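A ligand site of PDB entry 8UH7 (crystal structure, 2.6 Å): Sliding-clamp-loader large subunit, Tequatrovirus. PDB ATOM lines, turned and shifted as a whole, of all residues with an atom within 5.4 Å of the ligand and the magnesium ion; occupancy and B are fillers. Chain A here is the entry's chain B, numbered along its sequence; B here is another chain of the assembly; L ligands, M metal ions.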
ATOM      1  N   GLU A  17      24.721 -15.406   5.254  1.00  0.00           N
ATOM      2  CA  GLU A  17      23.539 -16.115   4.760  1.00  0.00           C
ATOM      3  C   GLU A  17      23.416 -16.060   3.245  1.00  0.00           C
ATOM      4  O   GLU A  17      22.800 -16.954   2.651  1.00  0.00           O
ATOM      5  CB  GLU A  17      22.262 -15.557   5.387  1.00  0.00           C
ATOM      6  CG  GLU A  17      22.058 -14.054   5.187  1.00  0.00           C
ATOM      7  CD  GLU A  17      22.288 -13.268   6.464  1.00  0.00           C
ATOM      8  OE1 GLU A  17      23.114 -13.718   7.289  1.00  0.00           O
ATOM      9  OE2 GLU A  17      21.645 -12.202   6.634  1.00  0.00           O
ATOM     10  N   GLN A  18      23.989 -15.045   2.602  1.00  0.00           N
ATOM     11  CA  GLN A  18      24.023 -14.947   1.149  1.00  0.00           C
ATOM     12  C   GLN A  18      25.226 -15.679   0.551  1.00  0.00           C
ATOM     13  O   GLN A  18      25.192 -16.011  -0.637  1.00  0.00           O
ATOM     14  CB  GLN A  18      24.063 -13.479   0.721  1.00  0.00           C
ATOM     15  CG  GLN A  18      23.375 -13.192  -0.606  1.00  0.00           C
ATOM     16  CD  GLN A  18      21.871 -13.180  -0.478  1.00  0.00           C
ATOM     17  OE1 GLN A  18      21.333 -12.985   0.611  1.00  0.00           O
ATOM     18  NE2 GLN A  18      21.178 -13.395  -1.592  1.00  0.00           N
ATOM     19  N   TYR A  20      26.462 -18.651   1.625  1.00  0.00           N
ATOM     20  CA  TYR A  20      26.253 -20.096   1.643  1.00  0.00           C
ATOM     21  C   TYR A  20      24.831 -20.455   1.254  1.00  0.00           C
ATOM     22  O   TYR A  20      24.150 -21.185   1.978  1.00  0.00           O
ATOM     23  CB  TYR A  20      26.599 -20.647   3.025  1.00  0.00           C
ATOM     24  CG  TYR A  20      28.059 -20.509   3.376  1.00  0.00           C
ATOM     25  CD1 TYR A  20      28.954 -21.539   3.126  1.00  0.00           C
ATOM     26  CD2 TYR A  20      28.544 -19.348   3.953  1.00  0.00           C
ATOM     27  CE1 TYR A  20      30.295 -21.421   3.450  1.00  0.00           C
ATOM     28  CE2 TYR A  20      29.884 -19.207   4.275  1.00  0.00           C
ATOM     29  CZ  TYR A  20      30.753 -20.253   4.024  1.00  0.00           C
ATOM     30  OH  TYR A  20      32.090 -20.122   4.344  1.00  0.00           O
ATOM     31  N   ARG A  21      24.367 -19.952   0.114  1.00  0.00           N
ATOM     32  CA  ARG A  21      23.044 -20.312  -0.377  1.00  0.00           C
ATOM     33  C   ARG A  21      23.115 -21.616  -1.149  1.00  0.00           C
ATOM     34  O   ARG A  21      23.856 -21.690  -2.147  1.00  0.00           O
ATOM     35  CB  ARG A  21      22.481 -19.204  -1.267  1.00  0.00           C
ATOM     36  CG  ARG A  21      21.105 -19.509  -1.826  1.00  0.00           C
ATOM     37  CD  ARG A  21      20.605 -18.377  -2.699  1.00  0.00           C
ATOM     38  NE  ARG A  21      20.387 -17.161  -1.925  1.00  0.00           N
ATOM     39  CZ  ARG A  21      19.243 -16.847  -1.325  1.00  0.00           C
ATOM     40  NH1 ARG A  21      18.215 -17.673  -1.401  1.00  0.00           N
ATOM     41  NH2 ARG A  21      19.131 -15.719  -0.646  1.00  0.00           N
ATOM     42  N   PRO A  22      22.404 -22.669  -0.740  1.00  0.00           N
ATOM     43  CA  PRO A  22      22.440 -23.929  -1.491  1.00  0.00           C
ATOM     44  C   PRO A  22      22.059 -23.733  -2.945  1.00  0.00           C
ATOM     45  O   PRO A  22      21.207 -22.906  -3.278  1.00  0.00           O
ATOM     46  CB  PRO A  22      21.427 -24.809  -0.746  1.00  0.00           C
ATOM     47  CG  PRO A  22      21.405 -24.259   0.639  1.00  0.00           C
ATOM     48  CD  PRO A  22      21.608 -22.774   0.497  1.00  0.00           C
ATOM     49  N   GLU A  27      21.137 -30.279  -1.572  1.00  0.00           N
ATOM     50  CA  GLU A  27      21.854 -29.529  -0.546  1.00  0.00           C
ATOM     51  C   GLU A  27      20.903 -28.835   0.420  1.00  0.00           C
ATOM     52  O   GLU A  27      21.271 -28.561   1.568  1.00  0.00           O
ATOM     53  CB  GLU A  27      22.787 -28.513  -1.194  1.00  0.00           C
ATOM     54  CG  GLU A  27      23.663 -27.738  -0.222  1.00  0.00           C
ATOM     55  CD  GLU A  27      24.482 -26.671  -0.920  1.00  0.00           C
ATOM     56  OE1 GLU A  27      24.490 -26.644  -2.159  1.00  0.00           O
ATOM     57  OE2 GLU A  27      25.119 -25.849  -0.215  1.00  0.00           O
ATOM     58  N   CYS A  28      19.673 -28.548  -0.014  1.00  0.00           N
ATOM     59  CA  CYS A  28      18.708 -27.869   0.835  1.00  0.00           C
ATOM     60  C   CYS A  28      18.212 -28.779   1.950  1.00  0.00           C
ATOM     61  O   CYS A  28      18.092 -30.003   1.776  1.00  0.00           O
ATOM     62  CB  CYS A  28      17.522 -27.371  -0.002  1.00  0.00           C
ATOM     63  SG  CYS A  28      17.988 -26.360  -1.423  1.00  0.00           S
ATOM     64  N   ILE A  29      17.928 -28.177   3.104  1.00  0.00           N
ATOM     65  CA  ILE A  29      17.436 -28.899   4.264  1.00  0.00           C
ATOM     66  C   ILE A  29      15.918 -28.753   4.277  1.00  0.00           C
ATOM     67  O   ILE A  29      15.388 -27.744   4.763  1.00  0.00           O
ATOM     68  CB  ILE A  29      18.073 -28.387   5.561  1.00  0.00           C
ATOM     69  CG1 ILE A  29      19.593 -28.467   5.469  1.00  0.00           C
ATOM     70  CG2 ILE A  29      17.562 -29.176   6.744  1.00  0.00           C
ATOM     71  CD1 ILE A  29      20.321 -27.849   6.639  1.00  0.00           C
ATOM     72  N   LEU A  30      15.223 -29.759   3.758  1.00  0.00           N
ATOM     73  CA  LEU A  30      13.774 -29.712   3.593  1.00  0.00           C
ATOM     74  C   LEU A  30      13.130 -30.888   4.321  1.00  0.00           C
ATOM     75  O   LEU A  30      13.824 -31.815   4.741  1.00  0.00           O
ATOM     76  CB  LEU A  30      13.423 -29.736   2.107  1.00  0.00           C
ATOM     77  CG  LEU A  30      14.123 -28.697   1.232  1.00  0.00           C
ATOM     78  CD1 LEU A  30      13.740 -28.870  -0.233  1.00  0.00           C
ATOM     79  CD2 LEU A  30      13.785 -27.291   1.717  1.00  0.00           C
ATOM     80  N   SER A  54       5.254 -19.938   2.277  1.00  0.00           N
ATOM     81  CA  SER A  54       5.400 -20.113   3.718  1.00  0.00           C
ATOM     82  C   SER A  54       5.462 -18.736   4.369  1.00  0.00           C
ATOM     83  O   SER A  54       6.323 -17.920   4.004  1.00  0.00           O
ATOM     84  CB  SER A  54       6.643 -20.922   4.072  1.00  0.00           C
ATOM     85  OG  SER A  54       7.830 -20.195   3.806  1.00  0.00           O
ATOM     86  N   SER A  56       6.519 -18.009   7.283  1.00  0.00           N
ATOM     87  CA  SER A  56       7.787 -17.924   8.009  1.00  0.00           C
ATOM     88  C   SER A  56       8.915 -17.629   7.037  1.00  0.00           C
ATOM     89  O   SER A  56       9.156 -18.423   6.121  1.00  0.00           O
ATOM     90  CB  SER A  56       8.061 -19.226   8.759  1.00  0.00           C
ATOM     91  OG  SER A  56       9.366 -19.220   9.299  1.00  0.00           O
ATOM     92  N   PRO A  57       9.627 -16.511   7.181  1.00  0.00           N
ATOM     93  CA  PRO A  57      10.703 -16.204   6.241  1.00  0.00           C
ATOM     94  C   PRO A  57      11.892 -17.129   6.420  1.00  0.00           C
ATOM     95  O   PRO A  57      12.062 -17.780   7.447  1.00  0.00           O
ATOM     96  CB  PRO A  57      11.058 -14.751   6.584  1.00  0.00           C
ATOM     97  CG  PRO A  57      10.682 -14.611   8.020  1.00  0.00           C
ATOM     98  CD  PRO A  57       9.479 -15.488   8.227  1.00  0.00           C
ATOM     99  N   GLY A  58      12.709 -17.183   5.373  1.00  0.00           N
ATOM    100  CA  GLY A  58      13.950 -17.958   5.409  1.00  0.00           C
ATOM    101  C   GLY A  58      13.791 -19.454   5.593  1.00  0.00           C
ATOM    102  O   GLY A  58      14.543 -20.053   6.364  1.00  0.00           O
ATOM    103  N   THR A  59      12.832 -20.062   4.898  1.00  0.00           N
ATOM    104  CA  THR A  59      12.702 -21.520   4.904  1.00  0.00           C
ATOM    105  C   THR A  59      13.344 -22.180   3.693  1.00  0.00           C
ATOM    106  O   THR A  59      13.777 -23.327   3.792  1.00  0.00           O
ATOM    107  CB  THR A  59      11.226 -21.924   4.976  1.00  0.00           C
ATOM    108  OG1 THR A  59      10.498 -21.296   3.920  1.00  0.00           O
ATOM    109  CG2 THR A  59      10.628 -21.512   6.306  1.00  0.00           C
ATOM    110  N   GLY A  60      13.411 -21.474   2.566  1.00  0.00           N
ATOM    111  CA  GLY A  60      14.130 -21.976   1.411  1.00  0.00           C
ATOM    112  C   GLY A  60      13.389 -21.872   0.092  1.00  0.00           C
ATOM    113  O   GLY A  60      13.743 -22.558  -0.871  1.00  0.00           O
ATOM    114  N   LYS A  61      12.374 -21.003   0.010  1.00  0.00           N
ATOM    115  CA  LYS A  61      11.558 -20.919  -1.194  1.00  0.00           C
ATOM    116  C   LYS A  61      12.355 -20.438  -2.403  1.00  0.00           C
ATOM    117  O   LYS A  61      12.373 -21.092  -3.446  1.00  0.00           O
ATOM    118  CB  LYS A  61      10.356 -20.006  -0.940  1.00  0.00           C
ATOM    119  CG  LYS A  61       9.484 -20.456   0.220  1.00  0.00           C
ATOM    120  CD  LYS A  61       8.355 -19.472   0.505  1.00  0.00           C
ATOM    121  CE  LYS A  61       8.863 -18.244   1.231  1.00  0.00           C
ATOM    122  NZ  LYS A  61       9.342 -18.584   2.596  1.00  0.00           N
ATOM    123  N   THR A  62      13.016 -19.293  -2.276  1.00  0.00           N
ATOM    124  CA  THR A  62      13.824 -18.782  -3.386  1.00  0.00           C
ATOM    125  C   THR A  62      14.981 -19.730  -3.701  1.00  0.00           C
ATOM    126  O   THR A  62      15.289 -19.976  -4.881  1.00  0.00           O
ATOM    127  CB  THR A  62      14.363 -17.388  -3.048  1.00  0.00           C
ATOM    128  OG1 THR A  62      13.311 -16.587  -2.465  1.00  0.00           O
ATOM    129  CG2 THR A  62      14.873 -16.694  -4.302  1.00  0.00           C
ATOM    130  N   THR A  63      15.618 -20.258  -2.664  1.00  0.00           N
ATOM    131  CA  THR A  63      16.700 -21.216  -2.861  1.00  0.00           C
ATOM    132  C   THR A  63      16.216 -22.433  -3.639  1.00  0.00           C
ATOM    133  O   THR A  63      16.867 -22.878  -4.582  1.00  0.00           O
ATOM    134  CB  THR A  63      17.286 -21.639  -1.507  1.00  0.00           C
ATOM    135  OG1 THR A  63      17.802 -20.491  -0.839  1.00  0.00           O
ATOM    136  CG2 THR A  63      18.387 -22.667  -1.698  1.00  0.00           C
ATOM    137  N   VAL A  64      15.053 -22.978  -3.253  1.00  0.00           N
ATOM    138  CA  VAL A  64      14.555 -24.190  -3.898  1.00  0.00           C
ATOM    139  C   VAL A  64      14.122 -23.902  -5.336  1.00  0.00           C
ATOM    140  O   VAL A  64      14.307 -24.734  -6.228  1.00  0.00           O
ATOM    141  CB  VAL A  64      13.433 -24.819  -3.060  1.00  0.00           C
ATOM    142  CG1 VAL A  64      12.570 -25.728  -3.917  1.00  0.00           C
ATOM    143  CG2 VAL A  64      14.027 -25.589  -1.902  1.00  0.00           C
ATOM    144  N   ASP A 112       9.731 -14.110  -7.779  1.00  0.00           N
ATOM    145  CA  ASP A 112      10.032 -14.172  -6.362  1.00  0.00           C
ATOM    146  C   ASP A 112       9.212 -13.145  -5.596  1.00  0.00           C
ATOM    147  O   ASP A 112       9.182 -11.961  -5.956  1.00  0.00           O
ATOM    148  CB  ASP A 112      11.529 -13.937  -6.142  1.00  0.00           C
ATOM    149  CG  ASP A 112      11.984 -14.372  -4.762  1.00  0.00           C
ATOM    150  OD1 ASP A 112      11.710 -15.538  -4.390  1.00  0.00           O
ATOM    151  OD2 ASP A 112      12.628 -13.559  -4.066  1.00  0.00           O
ATOM    152  N   GLU A 113       8.536 -13.593  -4.542  1.00  0.00           N
ATOM    153  CA  GLU A 113       7.731 -12.755  -3.660  1.00  0.00           C
ATOM    154  C   GLU A 113       6.678 -11.965  -4.461  1.00  0.00           C
ATOM    155  O   GLU A 113       6.786 -10.755  -4.687  1.00  0.00           O
ATOM    156  CB  GLU A 113       8.631 -11.822  -2.835  1.00  0.00           C
ATOM    157  CG  GLU A 113       9.816 -12.522  -2.172  1.00  0.00           C
ATOM    158  CD  GLU A 113       9.402 -13.602  -1.185  1.00  0.00           C
ATOM    159  OE1 GLU A 113       8.368 -13.431  -0.509  1.00  0.00           O
ATOM    160  OE2 GLU A 113      10.126 -14.632  -1.078  1.00  0.00           O
ATOM    161  N   THR A 142       7.087 -17.666  -5.711  1.00  0.00           N
ATOM    162  CA  THR A 142       7.330 -17.813  -4.290  1.00  0.00           C
ATOM    163  C   THR A 142       6.590 -16.711  -3.548  1.00  0.00           C
ATOM    164  O   THR A 142       6.397 -15.610  -4.078  1.00  0.00           O
ATOM    165  CB  THR A 142       8.833 -17.744  -3.950  1.00  0.00           C
ATOM    166  OG1 THR A 142       9.332 -16.428  -4.235  1.00  0.00           O
ATOM    167  CG2 THR A 142       9.614 -18.768  -4.768  1.00  0.00           C
ATOM    168  N   ASN A 144       5.105 -15.320   0.693  1.00  0.00           N
ATOM    169  CA  ASN A 144       4.898 -15.442   2.132  1.00  0.00           C
ATOM    170  C   ASN A 144       3.417 -15.537   2.488  1.00  0.00           C
ATOM    171  O   ASN A 144       2.996 -16.479   3.170  1.00  0.00           O
ATOM    172  CB  ASN A 144       5.527 -14.253   2.868  1.00  0.00           C
ATOM    173  CG  ASN A 144       7.024 -14.171   2.682  1.00  0.00           C
ATOM    174  OD1 ASN A 144       7.552 -13.107   2.364  1.00  0.00           O
ATOM    175  ND2 ASN A 144       7.710 -15.292   2.870  1.00  0.00           N
ATOM    176  N   MET A 177      20.805 -29.083  10.007  1.00  0.00           N
ATOM    177  CA  MET A 177      21.221 -27.698  10.112  1.00  0.00           C
ATOM    178  C   MET A 177      22.395 -27.536  11.066  1.00  0.00           C
ATOM    179  O   MET A 177      23.262 -26.690  10.844  1.00  0.00           O
ATOM    180  CB  MET A 177      20.046 -26.822  10.569  1.00  0.00           C
ATOM    181  CG  MET A 177      20.307 -25.327  10.387  1.00  0.00           C
ATOM    182  SD  MET A 177      20.690 -24.903   8.675  1.00  0.00           S
ATOM    183  CE  MET A 177      21.202 -23.192   8.833  1.00  0.00           C
ATOM    184  N   ARG A 180      25.305 -28.542   9.004  1.00  0.00           N
ATOM    185  CA  ARG A 180      25.619 -27.514   8.015  1.00  0.00           C
ATOM    186  C   ARG A 180      26.312 -26.319   8.652  1.00  0.00           C
ATOM    187  O   ARG A 180      27.273 -25.776   8.097  1.00  0.00           O
ATOM    188  CB  ARG A 180      24.349 -27.068   7.298  1.00  0.00           C
ATOM    189  CG  ARG A 180      24.603 -26.067   6.195  1.00  0.00           C
ATOM    190  CD  ARG A 180      23.347 -25.811   5.392  1.00  0.00           C
ATOM    191  NE  ARG A 180      23.636 -24.954   4.248  1.00  0.00           N
ATOM    192  CZ  ARG A 180      24.102 -25.412   3.091  1.00  0.00           C
ATOM    193  NH1 ARG A 180      24.325 -26.699   2.922  1.00  0.00           N
ATOM    194  NH2 ARG A 180      24.344 -24.567   2.084  1.00  0.00           N
ATOM    195  N   PHE A 209      16.112 -20.389   8.633  1.00  0.00           N
ATOM    196  CA  PHE A 209      17.517 -20.756   8.480  1.00  0.00           C
ATOM    197  C   PHE A 209      18.382 -19.535   8.182  1.00  0.00           C
ATOM    198  O   PHE A 209      19.537 -19.461   8.640  1.00  0.00           O
ATOM    199  CB  PHE A 209      17.672 -21.805   7.377  1.00  0.00           C
ATOM    200  CG  PHE A 209      17.145 -23.166   7.756  1.00  0.00           C
ATOM    201  CD1 PHE A 209      17.003 -23.515   9.093  1.00  0.00           C
ATOM    202  CD2 PHE A 209      16.803 -24.089   6.793  1.00  0.00           C
ATOM    203  CE1 PHE A 209      16.529 -24.761   9.445  1.00  0.00           C
ATOM    204  CE2 PHE A 209      16.328 -25.335   7.146  1.00  0.00           C
ATOM    205  CZ  PHE A 209      16.191 -25.671   8.472  1.00  0.00           C
ATOM    206  N   ARG A 210      17.856 -18.586   7.404  1.00  0.00           N
ATOM    207  CA  ARG A 210      18.581 -17.343   7.168  1.00  0.00           C
ATOM    208  C   ARG A 210      18.935 -16.662   8.491  1.00  0.00           C
ATOM    209  O   ARG A 210      20.082 -16.269   8.715  1.00  0.00           O
ATOM    210  CB  ARG A 210      17.747 -16.408   6.296  1.00  0.00           C
ATOM    211  CG  ARG A 210      18.394 -15.063   6.059  1.00  0.00           C
ATOM    212  CD  ARG A 210      17.417 -14.049   5.480  1.00  0.00           C
ATOM    213  NE  ARG A 210      17.019 -14.364   4.108  1.00  0.00           N
ATOM    214  CZ  ARG A 210      15.783 -14.698   3.750  1.00  0.00           C
ATOM    215  NH1 ARG A 210      14.813 -14.761   4.657  1.00  0.00           N
ATOM    216  NH2 ARG A 210      15.510 -14.964   2.480  1.00  0.00           N
ATOM    217  N   ILE A 213      21.806 -18.575  10.307  1.00  0.00           N
ATOM    218  CA  ILE A 213      23.157 -18.250   9.850  1.00  0.00           C
ATOM    219  C   ILE A 213      23.516 -16.816  10.249  1.00  0.00           C
ATOM    220  O   ILE A 213      24.684 -16.535  10.580  1.00  0.00           O
ATOM    221  CB  ILE A 213      23.278 -18.483   8.337  1.00  0.00           C
ATOM    222  CG1 ILE A 213      23.016 -19.962   8.017  1.00  0.00           C
ATOM    223  CG2 ILE A 213      24.652 -18.084   7.830  1.00  0.00           C
ATOM    224  CD1 ILE A 213      23.199 -20.308   6.552  1.00  0.00           C
ATOM    225  N   GLU B 131      18.337  -8.883  -1.399  1.00  0.00           N
ATOM    226  CA  GLU B 131      19.105 -10.052  -1.805  1.00  0.00           C
ATOM    227  C   GLU B 131      19.775  -9.884  -3.159  1.00  0.00           C
ATOM    228  O   GLU B 131      20.758 -10.569  -3.448  1.00  0.00           O
ATOM    229  CB  GLU B 131      18.210 -11.296  -1.830  1.00  0.00           C
ATOM    230  CG  GLU B 131      17.841 -11.813  -0.452  1.00  0.00           C
ATOM    231  CD  GLU B 131      16.879 -12.983  -0.497  1.00  0.00           C
ATOM    232  OE1 GLU B 131      16.073 -13.051  -1.458  1.00  0.00           O
ATOM    233  OE2 GLU B 131      16.924 -13.837   0.408  1.00  0.00           O
ATOM    234  N   PRO B 152       9.872 -10.686   6.988  1.00  0.00           N
ATOM    235  CA  PRO B 152      10.977 -11.000   6.070  1.00  0.00           C
ATOM    236  C   PRO B 152      12.143 -10.043   6.183  1.00  0.00           C
ATOM    237  O   PRO B 152      13.307 -10.474   6.157  1.00  0.00           O
ATOM    238  CB  PRO B 152      10.314 -10.937   4.687  1.00  0.00           C
ATOM    239  CG  PRO B 152       8.900 -11.281   4.942  1.00  0.00           C
ATOM    240  CD  PRO B 152       8.576 -10.673   6.276  1.00  0.00           C
ATOM    241  N   ARG B 156      16.062 -10.729   7.176  1.00  0.00           N
ATOM    242  CA  ARG B 156      17.190 -10.348   6.339  1.00  0.00           C
ATOM    243  C   ARG B 156      18.228  -9.498   7.061  1.00  0.00           C
ATOM    244  O   ARG B 156      19.339  -9.340   6.547  1.00  0.00           O
ATOM    245  CB  ARG B 156      16.697  -9.585   5.100  1.00  0.00           C
ATOM    246  CG  ARG B 156      16.171 -10.483   4.008  1.00  0.00           C
ATOM    247  CD  ARG B 156      15.211  -9.759   3.079  1.00  0.00           C
ATOM    248  NE  ARG B 156      14.777 -10.636   1.994  1.00  0.00           N
ATOM    249  CZ  ARG B 156      13.890 -11.618   2.153  1.00  0.00           C
ATOM    250  NH1 ARG B 156      13.342 -11.844   3.334  1.00  0.00           N
ATOM    251  NH2 ARG B 156      13.546 -12.377   1.108  1.00  0.00           N
HETATM  252  P1  LIG L   1      15.844 -18.243   1.041  1.00  0.00           P
HETATM  253  P2  LIG L   1      13.205 -17.796   1.750  1.00  0.00           P
HETATM  254 BE1  LIG L   1      11.823 -15.416   2.318  1.00  0.00          BE
HETATM  255  C1  LIG L   1      17.976 -17.750   2.414  1.00  0.00           C
HETATM  256  O1  LIG L   1      17.118 -18.670   1.830  1.00  0.00           O
HETATM  257  C2  LIG L   1      19.179 -18.271   3.106  1.00  0.00           C
HETATM  258  O2  LIG L   1      18.812 -18.971   4.249  1.00  0.00           O
HETATM  259  C3  LIG L   1      19.882 -19.245   2.252  1.00  0.00           C
HETATM  260  O3  LIG L   1      20.858 -18.666   1.434  1.00  0.00           O
HETATM  261  C4  LIG L   1      20.401 -20.198   3.153  1.00  0.00           C
HETATM  262  O4  LIG L   1      21.663 -19.885   3.628  1.00  0.00           O
HETATM  263  C5  LIG L   1      19.443 -20.218   4.259  1.00  0.00           C
HETATM  264  N1  LIG L   1      18.630 -25.266   3.464  1.00  0.00           N
HETATM  265  O5  LIG L   1      15.902 -16.896   0.301  1.00  0.00           O
HETATM  266  O6  LIG L   1      12.326 -19.053   1.896  1.00  0.00           O
HETATM  267  F1  LIG L   1      11.851 -15.372   0.804  1.00  0.00           F
HETATM  268  C6  LIG L   1      19.792 -24.671   3.679  1.00  0.00           C
HETATM  269  O7  LIG L   1      15.568 -19.367   0.027  1.00  0.00           O
HETATM  270  O8  LIG L   1      13.167 -17.202   0.330  1.00  0.00           O
HETATM  271  F2  LIG L   1      12.351 -14.181   2.870  1.00  0.00           F
HETATM  272  N2  LIG L   1      19.847 -23.343   3.870  1.00  0.00           N
HETATM  273  O9  LIG L   1      14.635 -18.253   2.113  1.00  0.00           O
HETATM  274  O10 LIG L   1      12.740 -16.621   2.760  1.00  0.00           O
HETATM  275  F3  LIG L   1      10.391 -15.551   2.805  1.00  0.00           F
HETATM  276  C7  LIG L   1      18.727 -22.576   3.845  1.00  0.00           C
HETATM  277  C8  LIG L   1      17.519 -23.189   3.618  1.00  0.00           C
HETATM  278  C9  LIG L   1      17.490 -24.555   3.429  1.00  0.00           C
HETATM  279  N3  LIG L   1      16.244 -25.203   3.200  1.00  0.00           N
HETATM  280  N4  LIG L   1      16.591 -22.236   3.655  1.00  0.00           N
HETATM  281  C10 LIG L   1      17.174 -21.072   3.878  1.00  0.00           C
HETATM  282  N5  LIG L   1      18.483 -21.260   4.003  1.00  0.00           N
HETATM  283 MG    MG M   1      12.712 -15.109  -1.025  1.00  0.00          MG
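The guanidinium group of Arg 156 of chain B is in hydrogen-bond range of a fluorine (F2) of the ligand (2.6 Å). O of Ile 29 lies within hydrogen-bond range of N3 of the ligand (3.1 Å). NH1 of Arg 21 lies within salt-bridge range of O5 of the ligand (3.0 Å). N of Gly 60 lies within hydrogen-bond range of O6 of the ligand (2.7 Å). OG1 of Thr 63 is in hydrogen-bond range of O7 of the ligand. The backbone NH (N) of Thr 63 sits at hydrogen-bond distance from an oxygen (O7) of the ligand. The backbone NH (N) of Ile 29 lies within hydrogen-bond range of a nitrogen (N1) of the ligand (3.0 Å). O7 of the ligand is in hydrogen-bond range of N of Thr 62 (3.4 Å). The guanidinium group of Arg 210 lies within salt-bridge range of an oxygen (O5) of the ligand (2.9 Å). The backbone NH (N) of Thr 59 is in hydrogen-bond range of an oxygen (O6) of the ligand (3.2 Å). O4 of the ligand lies within hydrogen-bond range of O of Tyr 20 (3.3 Å). The side-chain amide nitrogen of Asn 144 sits at hydrogen-bond distance from a fluorine (F3) of the ligand (2.7 Å). O of Glu 17 sits at hydrogen-bond distance from O3 of the ligand (2.9 Å). An oxygen (O2) of the ligand is in hydrogen-bond range of the backbone NH (N) of Arg 210, at 3.3 Å. An oxygen (O10) of the ligand lies close to the backbone NH of Gly 58 (2.7 Å). The backbone carbonyl oxygen (O) of Thr 59 is in hydrogen-bond range of a nitrogen (N3) of the ligand (3.2 Å). The backbone NH (N) of Lys 61 sits at hydrogen-bond distance from an oxygen (O6) of the ligand (2.7 Å). NZ of Lys 61 lies within salt-bridge range of O6 of the ligand (3.1 Å).
NZ of Lys 61 sits at hydrogen-bond distance from OG of Ser 54, at 2.5 Å. NH1 of Arg 21 sits at hydrogen-bond distance from OG1 of Thr 63. NZ of Lys 61 is in hydrogen-bond range of OG1 of Thr 59, at 3.2 Å. NH2 of Arg 156 of chain B lies within salt-bridge range of OE1 of Glu 131 of chain B (3.7 Å). OG1 of Thr 59 is in hydrogen-bond range of OG of Ser 54 (2.9 Å). The backbone carbonyl oxygen of Gly 58 is in hydrogen-bond range of the backbone NH of Phe 209, at 2.8 Å. OG1 of Thr 142 is in hydrogen-bond range of OD1 of Asp 112 (2.5 Å). OE2 of Glu 131 of chain B lies within salt-bridge range of NH2 of Arg 210 (2.8 Å).
An oxygen (O5) of the ligand lies close to the side-chain carboxylate of Glu 131 of chain B, 3.2 Å away. Pro 22 touches the ligand (CG to C6, 3.5 Å). CA of Cys 28 touches N1 of the ligand, 3.7 Å away. Leu 30 touches the ligand (CD2 to N3, 3.6 Å). Pro 57 touches the ligand. NE of Arg 180 touches C6 of the ligand, 3.9 Å away. Phe 209 touches the ligand (CD2 to C8, 3.4 Å). Ile 213 touches the ligand (CD1 to O4, 3.3 Å). 22 residues have an atom within 4 Å of the ligand: Glu 17, Tyr 20, Arg 21, Pro 22, Cys 28, Ile 29, Leu 30, Pro 57, Gly 58, Thr 59, Gly 60, Lys 61, Thr 62, Thr 63, Glu 113, Asn 144, Arg 180, Phe 209, Arg 210, Ile 213, Glu 131 of chain B and Arg 156 of chain B. The nearest printed residue that does not touch the ligand is Pro 152 of chain B (4.2 Å).
Residues that only touch the magnesium ion: Asp 112 (3.4 Å), Glu 131 of chain B (3.96 Å) and Arg 156 of chain B (3.6 Å). Within 4 Å of the magnesium ion: Thr 62, Asp 112, Glu 113, Glu 131 of chain B and Arg 156 of chain B.
The magnesium ion is bound by F1 of the ligand (2.0 Å), OG1 of Thr 62 (2.1 Å) and O8 of the ligand (2.5 Å). The magnesium ion has three donor atoms within binding distance. Slightly farther from the magnesium ion lies the side-chain carboxylate (OE2) of Glu 113 (2.6 Å).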
